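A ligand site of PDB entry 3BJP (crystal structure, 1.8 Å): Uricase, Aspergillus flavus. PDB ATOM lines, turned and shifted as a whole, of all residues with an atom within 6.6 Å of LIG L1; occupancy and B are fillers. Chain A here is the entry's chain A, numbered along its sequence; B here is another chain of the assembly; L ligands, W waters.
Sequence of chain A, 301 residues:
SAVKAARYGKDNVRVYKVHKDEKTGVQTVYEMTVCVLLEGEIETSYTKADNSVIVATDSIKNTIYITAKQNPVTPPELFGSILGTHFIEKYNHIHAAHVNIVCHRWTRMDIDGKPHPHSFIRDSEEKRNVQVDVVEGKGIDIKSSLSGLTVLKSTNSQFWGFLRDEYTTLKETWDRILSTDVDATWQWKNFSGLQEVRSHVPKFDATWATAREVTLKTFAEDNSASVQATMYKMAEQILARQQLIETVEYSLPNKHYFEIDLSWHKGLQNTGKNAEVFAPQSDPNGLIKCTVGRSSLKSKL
Merely in contact with LIG L1: Phe 159 (3.3 Å), Ser 226 (3.4 Å), Leu 170 (3.5 Å), Ala 56 of chain B (3.6 Å), Ile 54 of chain B (3.6 Å), Tyr 8 of chain B (3.7 Å) and Ile 288 (3.9 Å).
Hydrophobic or aromatic side chains within 4 Å of LIG L1: Phe 159, Leu 170, Val 227, Ile 288, Tyr 8 of chain B, Ile 54 of chain B and Ala 56 of chain B.
Of the 26 residues printed, 13 come within 4 Å of LIG L1.
The nearest printed residue that does not touch LIG L1 is His 256 (4.8 Å).
The backbone NH of Asn 254 lies within hydrogen-bond range of the backbone carbonyl oxygen of Gly 286 (2.7 Å).
The backbone carbonyl oxygen (O) of Ser 226 sits at hydrogen-bond distance from the side-chain hydroxyl (OG) of Ser 224 (2.7 Å).
NE2 of His 256 lies within hydrogen-bond range of O of Asn 254 (3.4 Å).
N of Arg 176 lies within hydrogen-bond range of O of Ser 157, 2.9 Å away.
The side-chain hydroxyl of Tyr 8 of chain B lies within hydrogen-bond range of the backbone carbonyl oxygen of Val 55 of chain B (2.5 Å).
N of Gln 228 sits close to OG of Ser 226, 3.5 Å away.
Water W1 bridges O3 of LIG L1 (2.7 Å) and NZ of Lys 10 of chain B (3.3 Å).
Water W2 bridges N3 of LIG L1 and NH1 of Arg 176.
A nitrogen (N2) of LIG L1 sits close to a nitrogen (N1) of LG2 L2.
N4 of LIG L1 is in hydrogen-bond range of OG1 of Thr 57 of chain B.
ND2 of Asn 254 sits close to N2 of LIG L1 (3.5 Å).
O1 of LIG L1 lies within hydrogen-bond range of NH2 of Arg 176, at 3.0 Å.
NE2 of Gln 228 sits at hydrogen-bond distance from O2 of LIG L1, 2.8 Å away.
A nitrogen (N1) of LG2 L2 sits at hydrogen-bond distance from the side-chain amide nitrogen (ND2) of Asn 254, 2.9 Å away.
An oxygen (O3) of LIG L1 lies within hydrogen-bond range of the backbone NH of Thr 57 of chain B (3.2 Å).
O3 of LIG L1 is in hydrogen-bond range of N of Asp 58 of chain B (2.8 Å).
An oxygen (O1) of LIG L1 lies within hydrogen-bond range of the backbone NH (N) of Val 227 (2.8 Å).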
ATOM      1  N   SER A 157     -35.567  -1.424  22.268  1.00  0.00           N
ATOM      2  CA  SER A 157     -34.521  -1.100  21.322  1.00  0.00           C
ATOM      3  C   SER A 157     -35.081  -0.125  20.281  1.00  0.00           C
ATOM      4  O   SER A 157     -36.218  -0.227  19.840  1.00  0.00           O
ATOM      5  CB  SER A 157     -33.961  -2.365  20.671  1.00  0.00           C
ATOM      6  OG  SER A 157     -33.046  -1.995  19.662  1.00  0.00           O
ATOM      7  N   GLN A 158     -34.255   0.839  19.922  1.00  0.00           N
ATOM      8  CA  GLN A 158     -34.685   1.878  19.014  1.00  0.00           C
ATOM      9  C   GLN A 158     -33.577   2.233  18.033  1.00  0.00           C
ATOM     10  O   GLN A 158     -32.397   1.972  18.269  1.00  0.00           O
ATOM     11  CB  GLN A 158     -35.095   3.134  19.795  1.00  0.00           C
ATOM     12  CG  GLN A 158     -36.088   2.949  20.912  1.00  0.00           C
ATOM     13  CD  GLN A 158     -36.338   4.242  21.679  1.00  0.00           C
ATOM     14  OE1 GLN A 158     -36.460   5.326  21.110  1.00  0.00           O
ATOM     15  NE2 GLN A 158     -36.408   4.122  22.995  1.00  0.00           N
ATOM     16  N   PHE A 159     -33.957   2.836  16.912  1.00  0.00           N
ATOM     17  CA  PHE A 159     -32.998   3.382  15.982  1.00  0.00           C
ATOM     18  C   PHE A 159     -33.658   4.443  15.108  1.00  0.00           C
ATOM     19  O   PHE A 159     -34.346   4.147  14.135  1.00  0.00           O
ATOM     20  CB  PHE A 159     -32.359   2.284  15.133  1.00  0.00           C
ATOM     21  CG  PHE A 159     -31.144   2.740  14.347  1.00  0.00           C
ATOM     22  CD1 PHE A 159     -30.049   3.281  15.025  1.00  0.00           C
ATOM     23  CD2 PHE A 159     -31.074   2.626  12.988  1.00  0.00           C
ATOM     24  CE1 PHE A 159     -28.950   3.683  14.281  1.00  0.00           C
ATOM     25  CE2 PHE A 159     -29.975   3.018  12.223  1.00  0.00           C
ATOM     26  CZ  PHE A 159     -28.899   3.546  12.917  1.00  0.00           C
ATOM     27  N   PHE A 162     -30.688   8.655  12.343  1.00  0.00           N
ATOM     28  CA  PHE A 162     -29.539   8.372  11.492  1.00  0.00           C
ATOM     29  C   PHE A 162     -29.610   9.178  10.196  1.00  0.00           C
ATOM     30  O   PHE A 162     -30.707   9.640   9.856  1.00  0.00           O
ATOM     31  CB  PHE A 162     -29.443   6.884  11.144  1.00  0.00           C
ATOM     32  CG  PHE A 162     -30.746   6.297  10.623  1.00  0.00           C
ATOM     33  CD1 PHE A 162     -31.645   5.761  11.509  1.00  0.00           C
ATOM     34  CD2 PHE A 162     -31.001   6.307   9.272  1.00  0.00           C
ATOM     35  CE1 PHE A 162     -32.829   5.219  11.046  1.00  0.00           C
ATOM     36  CE2 PHE A 162     -32.192   5.772   8.805  1.00  0.00           C
ATOM     37  CZ  PHE A 162     -33.101   5.243   9.697  1.00  0.00           C
ATOM     38  N   LEU A 170     -34.335   2.686   4.962  1.00  0.00           N
ATOM     39  CA  LEU A 170     -34.706   2.239   6.279  1.00  0.00           C
ATOM     40  C   LEU A 170     -35.582   3.249   6.981  1.00  0.00           C
ATOM     41  O   LEU A 170     -35.275   4.447   7.038  1.00  0.00           O
ATOM     42  CB  LEU A 170     -33.450   1.977   7.119  1.00  0.00           C
ATOM     43  CG  LEU A 170     -33.686   1.475   8.533  1.00  0.00           C
ATOM     44  CD1 LEU A 170     -34.236   0.055   8.505  1.00  0.00           C
ATOM     45  CD2 LEU A 170     -32.422   1.542   9.376  1.00  0.00           C
ATOM     46  N   ARG A 176     -38.032  -1.964  18.340  1.00  0.00           N
ATOM     47  CA  ARG A 176     -37.562  -3.077  17.509  1.00  0.00           C
ATOM     48  C   ARG A 176     -36.945  -4.177  18.362  1.00  0.00           C
ATOM     49  O   ARG A 176     -36.697  -4.016  19.550  1.00  0.00           O
ATOM     50  CB  ARG A 176     -36.529  -2.621  16.488  1.00  0.00           C
ATOM     51  CG  ARG A 176     -35.236  -2.139  17.126  1.00  0.00           C
ATOM     52  CD  ARG A 176     -34.202  -1.783  16.054  1.00  0.00           C
ATOM     53  NE  ARG A 176     -32.905  -1.588  16.689  1.00  0.00           N
ATOM     54  CZ  ARG A 176     -31.749  -1.319  16.109  1.00  0.00           C
ATOM     55  NH1 ARG A 176     -31.616  -1.203  14.806  1.00  0.00           N
ATOM     56  NH2 ARG A 176     -30.680  -1.178  16.895  1.00  0.00           N
ATOM     57  N   LEU A 178     -33.748  -6.442  19.187  1.00  0.00           N
ATOM     58  CA  LEU A 178     -32.296  -6.400  19.095  1.00  0.00           C
ATOM     59  C   LEU A 178     -31.724  -7.750  19.537  1.00  0.00           C
ATOM     60  O   LEU A 178     -31.963  -8.185  20.664  1.00  0.00           O
ATOM     61  CB  LEU A 178     -31.709  -5.295  19.947  1.00  0.00           C
ATOM     62  CG  LEU A 178     -30.180  -5.198  19.992  1.00  0.00           C
ATOM     63  CD1 LEU A 178     -29.595  -5.007  18.602  1.00  0.00           C
ATOM     64  CD2 LEU A 178     -29.734  -4.059  20.897  1.00  0.00           C
ATOM     65  N   SER A 224     -31.983   0.992  24.484  1.00  0.00           N
ATOM     66  CA  SER A 224     -30.946   1.234  23.514  1.00  0.00           C
ATOM     67  C   SER A 224     -31.342   2.163  22.377  1.00  0.00           C
ATOM     68  O   SER A 224     -32.350   1.964  21.684  1.00  0.00           O
ATOM     69  CB  SER A 224     -30.477  -0.105  22.904  1.00  0.00           C
ATOM     70  OG  SER A 224     -29.621   0.092  21.791  1.00  0.00           O
ATOM     71  N   ALA A 225     -30.520   3.170  22.171  1.00  0.00           N
ATOM     72  CA  ALA A 225     -30.636   4.149  21.104  1.00  0.00           C
ATOM     73  C   ALA A 225     -29.989   3.648  19.816  1.00  0.00           C
ATOM     74  O   ALA A 225     -30.201   4.165  18.723  1.00  0.00           O
ATOM     75  CB  ALA A 225     -29.972   5.467  21.517  1.00  0.00           C
ATOM     76  N   SER A 226     -29.161   2.621  19.976  1.00  0.00           N
ATOM     77  CA  SER A 226     -28.466   1.944  18.910  1.00  0.00           C
ATOM     78  C   SER A 226     -27.465   0.929  19.503  1.00  0.00           C
ATOM     79  O   SER A 226     -27.245   0.949  20.710  1.00  0.00           O
ATOM     80  CB  SER A 226     -27.721   2.907  17.978  1.00  0.00           C
ATOM     81  OG  SER A 226     -26.642   3.467  18.701  1.00  0.00           O
ATOM     82  N   VAL A 227     -26.919   0.078  18.642  1.00  0.00           N
ATOM     83  CA  VAL A 227     -25.930  -0.890  19.107  1.00  0.00           C
ATOM     84  C   VAL A 227     -24.693  -0.149  19.616  1.00  0.00           C
ATOM     85  O   VAL A 227     -24.144  -0.496  20.657  1.00  0.00           O
ATOM     86  CB  VAL A 227     -25.598  -1.868  17.974  1.00  0.00           C
ATOM     87  CG1 VAL A 227     -24.535  -2.878  18.385  1.00  0.00           C
ATOM     88  CG2 VAL A 227     -26.875  -2.605  17.557  1.00  0.00           C
ATOM     89  N   GLN A 228     -24.307   0.869  18.871  1.00  0.00           N
ATOM     90  CA  GLN A 228     -23.169   1.728  19.212  1.00  0.00           C
ATOM     91  C   GLN A 228     -23.239   2.231  20.649  1.00  0.00           C
ATOM     92  O   GLN A 228     -22.321   2.058  21.454  1.00  0.00           O
ATOM     93  CB  GLN A 228     -23.105   2.885  18.218  1.00  0.00           C
ATOM     94  CG  GLN A 228     -22.668   2.577  16.809  1.00  0.00           C
ATOM     95  CD  GLN A 228     -23.784   2.156  15.863  1.00  0.00           C
ATOM     96  OE1 GLN A 228     -24.803   1.619  16.290  1.00  0.00           O
ATOM     97  NE2 GLN A 228     -23.596   2.382  14.575  1.00  0.00           N
ATOM     98  N   ASN A 254     -25.556  -7.098  14.306  1.00  0.00           N
ATOM     99  CA  ASN A 254     -26.967  -6.807  14.519  1.00  0.00           C
ATOM    100  C   ASN A 254     -27.760  -7.878  13.739  1.00  0.00           C
ATOM    101  O   ASN A 254     -27.827  -7.738  12.533  1.00  0.00           O
ATOM    102  CB  ASN A 254     -27.356  -5.414  14.060  1.00  0.00           C
ATOM    103  CG  ASN A 254     -28.671  -4.923  14.633  1.00  0.00           C
ATOM    104  OD1 ASN A 254     -29.441  -5.702  15.190  1.00  0.00           O
ATOM    105  ND2 ASN A 254     -28.944  -3.620  14.483  1.00  0.00           N
ATOM    106  N   HIS A 256     -30.678  -9.128  12.395  1.00  0.00           N
ATOM    107  CA  HIS A 256     -31.951  -8.471  12.138  1.00  0.00           C
ATOM    108  C   HIS A 256     -33.145  -9.435  12.133  1.00  0.00           C
ATOM    109  O   HIS A 256     -33.043 -10.534  11.608  1.00  0.00           O
ATOM    110  CB  HIS A 256     -31.875  -7.748  10.799  1.00  0.00           C
ATOM    111  CG  HIS A 256     -30.724  -6.798  10.652  1.00  0.00           C
ATOM    112  ND1 HIS A 256     -30.575  -5.673  11.443  1.00  0.00           N
ATOM    113  CD2 HIS A 256     -29.669  -6.810   9.807  1.00  0.00           C
ATOM    114  CE1 HIS A 256     -29.471  -5.047  11.077  1.00  0.00           C
ATOM    115  NE2 HIS A 256     -28.896  -5.701  10.094  1.00  0.00           N
ATOM    116  N   GLY A 286     -25.785  -6.081  10.203  1.00  0.00           N
ATOM    117  CA  GLY A 286     -24.938  -4.948  10.599  1.00  0.00           C
ATOM    118  C   GLY A 286     -23.830  -5.506  11.490  1.00  0.00           C
ATOM    119  O   GLY A 286     -24.029  -6.525  12.152  1.00  0.00           O
ATOM    120  N   ILE A 288     -20.976  -3.886  14.237  1.00  0.00           N
ATOM    121  CA  ILE A 288     -20.631  -2.698  14.993  1.00  0.00           C
ATOM    122  C   ILE A 288     -19.477  -2.997  15.941  1.00  0.00           C
ATOM    123  O   ILE A 288     -19.563  -3.938  16.739  1.00  0.00           O
ATOM    124  CB  ILE A 288     -21.835  -2.182  15.783  1.00  0.00           C
ATOM    125  CG1 ILE A 288     -23.155  -2.285  15.044  1.00  0.00           C
ATOM    126  CG2 ILE A 288     -21.596  -0.742  16.255  1.00  0.00           C
ATOM    127  CD1 ILE A 288     -23.281  -1.576  13.731  1.00  0.00           C
ATOM    128  N   TYR B   8     -17.870   0.458  11.791  1.00  0.00           N
ATOM    129  CA  TYR B   8     -19.217  -0.154  11.771  1.00  0.00           C
ATOM    130  C   TYR B   8     -19.587  -0.291  10.302  1.00  0.00           C
ATOM    131  O   TYR B   8     -19.144   0.408   9.404  1.00  0.00           O
ATOM    132  CB  TYR B   8     -20.209   0.675  12.627  1.00  0.00           C
ATOM    133  CG  TYR B   8     -20.828   1.708  11.706  1.00  0.00           C
ATOM    134  CD1 TYR B   8     -20.066   2.832  11.368  1.00  0.00           C
ATOM    135  CD2 TYR B   8     -22.113   1.591  11.173  1.00  0.00           C
ATOM    136  CE1 TYR B   8     -20.570   3.815  10.538  1.00  0.00           C
ATOM    137  CE2 TYR B   8     -22.601   2.564  10.318  1.00  0.00           C
ATOM    138  CZ  TYR B   8     -21.845   3.676  10.000  1.00  0.00           C
ATOM    139  OH  TYR B   8     -22.363   4.621   9.149  1.00  0.00           O
ATOM    140  N   GLY B   9     -20.516  -1.223  10.022  1.00  0.00           N
ATOM    141  CA  GLY B   9     -20.956  -1.356   8.645  1.00  0.00           C
ATOM    142  C   GLY B   9     -21.850  -2.595   8.472  1.00  0.00           C
ATOM    143  O   GLY B   9     -22.480  -3.017   9.427  1.00  0.00           O
ATOM    144  N   LYS B  10     -21.849  -3.105   7.257  1.00  0.00           N
ATOM    145  CA  LYS B  10     -22.655  -4.267   6.901  1.00  0.00           C
ATOM    146  C   LYS B  10     -21.745  -5.427   6.498  1.00  0.00           C
ATOM    147  O   LYS B  10     -20.819  -5.255   5.712  1.00  0.00           O
ATOM    148  CB  LYS B  10     -23.581  -3.943   5.742  1.00  0.00           C
ATOM    149  CG  LYS B  10     -24.824  -4.829   5.688  1.00  0.00           C
ATOM    150  CD  LYS B  10     -25.772  -4.504   6.817  1.00  0.00           C
ATOM    151  CE  LYS B  10     -27.203  -4.950   6.511  1.00  0.00           C
ATOM    152  NZ  LYS B  10     -28.193  -4.427   7.482  1.00  0.00           N
ATOM    153  N   ASN B  51     -27.077   9.698  16.458  1.00  0.00           N
ATOM    154  CA  ASN B  51     -27.097   8.886  15.233  1.00  0.00           C
ATOM    155  C   ASN B  51     -26.945   9.692  13.963  1.00  0.00           C
ATOM    156  O   ASN B  51     -26.899   9.122  12.868  1.00  0.00           O
ATOM    157  CB  ASN B  51     -28.417   8.086  15.236  1.00  0.00           C
ATOM    158  CG  ASN B  51     -28.359   6.997  16.297  1.00  0.00           C
ATOM    159  OD1 ASN B  51     -27.279   6.541  16.684  1.00  0.00           O
ATOM    160  ND2 ASN B  51     -29.516   6.576  16.757  1.00  0.00           N
ATOM    161  N   ILE B  54     -24.370   8.583  11.693  1.00  0.00           N
ATOM    162  CA  ILE B  54     -24.420   7.213  11.182  1.00  0.00           C
ATOM    163  C   ILE B  54     -25.087   7.115   9.828  1.00  0.00           C
ATOM    164  O   ILE B  54     -26.239   7.528   9.656  1.00  0.00           O
ATOM    165  CB  ILE B  54     -25.115   6.284  12.202  1.00  0.00           C
ATOM    166  CG1 ILE B  54     -24.430   6.242  13.571  1.00  0.00           C
ATOM    167  CG2 ILE B  54     -25.219   4.877  11.635  1.00  0.00           C
ATOM    168  CD1 ILE B  54     -23.027   5.678  13.498  1.00  0.00           C
ATOM    169  N   VAL B  55     -24.344   6.576   8.878  1.00  0.00           N
ATOM    170  CA  VAL B  55     -24.847   6.092   7.600  1.00  0.00           C
ATOM    171  C   VAL B  55     -25.372   4.679   7.932  1.00  0.00           C
ATOM    172  O   VAL B  55     -24.542   3.812   8.167  1.00  0.00           O
ATOM    173  CB  VAL B  55     -23.807   6.072   6.495  1.00  0.00           C
ATOM    174  CG1 VAL B  55     -24.301   5.463   5.193  1.00  0.00           C
ATOM    175  CG2 VAL B  55     -23.339   7.512   6.214  1.00  0.00           C
ATOM    176  N   ALA B  56     -26.696   4.529   7.998  1.00  0.00           N
ATOM    177  CA  ALA B  56     -27.322   3.261   8.403  1.00  0.00           C
ATOM    178  C   ALA B  56     -26.677   2.095   7.683  1.00  0.00           C
ATOM    179  O   ALA B  56     -26.326   2.197   6.512  1.00  0.00           O
ATOM    180  CB  ALA B  56     -28.821   3.270   8.141  1.00  0.00           C
ATOM    181  N   THR B  57     -26.504   0.978   8.414  1.00  0.00           N
ATOM    182  CA  THR B  57     -25.899  -0.157   7.719  1.00  0.00           C
ATOM    183  C   THR B  57     -26.864  -0.644   6.631  1.00  0.00           C
ATOM    184  O   THR B  57     -26.439  -1.161   5.620  1.00  0.00           O
ATOM    185  CB  THR B  57     -25.511  -1.299   8.657  1.00  0.00           C
ATOM    186  OG1 THR B  57     -26.655  -1.845   9.298  1.00  0.00           O
ATOM    187  CG2 THR B  57     -24.623  -0.764   9.786  1.00  0.00           C
ATOM    188  N   ASP B  58     -28.150  -0.414   6.863  1.00  0.00           N
ATOM    189  CA  ASP B  58     -29.121  -0.758   5.830  1.00  0.00           C
ATOM    190  C   ASP B  58     -28.819   0.022   4.562  1.00  0.00           C
ATOM    191  O   ASP B  58     -28.877  -0.481   3.454  1.00  0.00           O
ATOM    192  CB  ASP B  58     -30.546  -0.507   6.331  1.00  0.00           C
ATOM    193  CG  ASP B  58     -31.554  -1.009   5.305  1.00  0.00           C
ATOM    194  OD1 ASP B  58     -31.880  -2.208   5.347  1.00  0.00           O
ATOM    195  OD2 ASP B  58     -31.989  -0.215   4.438  1.00  0.00           O
ATOM    196  N   SER B  59     -28.462   1.313   4.764  1.00  0.00           N
ATOM    197  CA  SER B  59     -28.093   2.133   3.622  1.00  0.00           C
ATOM    198  C   SER B  59     -26.803   1.693   2.959  1.00  0.00           C
ATOM    199  O   SER B  59     -26.608   1.765   1.747  1.00  0.00           O
ATOM    200  CB  SER B  59     -27.998   3.614   4.049  1.00  0.00           C
ATOM    201  OG  SER B  59     -29.177   3.979   4.729  1.00  0.00           O
HETATM  202  N1  LIG L   1     -26.847   0.754  14.359  1.00  0.00           N
HETATM  203  C1  LIG L   1     -27.991   0.201  14.894  1.00  0.00           C
HETATM  204  C2  LIG L   1     -26.542   0.977  13.038  1.00  0.00           C
HETATM  205  N2  LIG L   1     -28.977  -0.187  14.021  1.00  0.00           N
HETATM  206  O1  LIG L   1     -28.082   0.079  16.096  1.00  0.00           O
HETATM  207  C3  LIG L   1     -28.748  -0.002  12.688  1.00  0.00           C
HETATM  208  C4  LIG L   1     -27.625   0.595  12.162  1.00  0.00           C
HETATM  209  N3  LIG L   1     -29.577  -0.277  11.621  1.00  0.00           N
HETATM  210  O2  LIG L   1     -25.485   1.464  12.705  1.00  0.00           O
HETATM  211  N4  LIG L   1     -27.670   0.642  10.847  1.00  0.00           N
HETATM  212  C5  LIG L   1     -28.850   0.123  10.542  1.00  0.00           C
HETATM  213  O3  LIG L   1     -29.335  -0.023   9.386  1.00  0.00           O
HETATM  214  C1  LG2 L   2     -26.729  -2.573  12.006  1.00  0.00           C
HETATM  215  N1  LG2 L   2     -26.689  -2.347  13.177  1.00  0.00           N
HETATM  216  O   HOH W   1     -30.272  -2.500   9.200  1.00  0.00           O
HETATM  217  O   HOH W   2     -31.901  -2.025  11.715  1.00  0.00           O
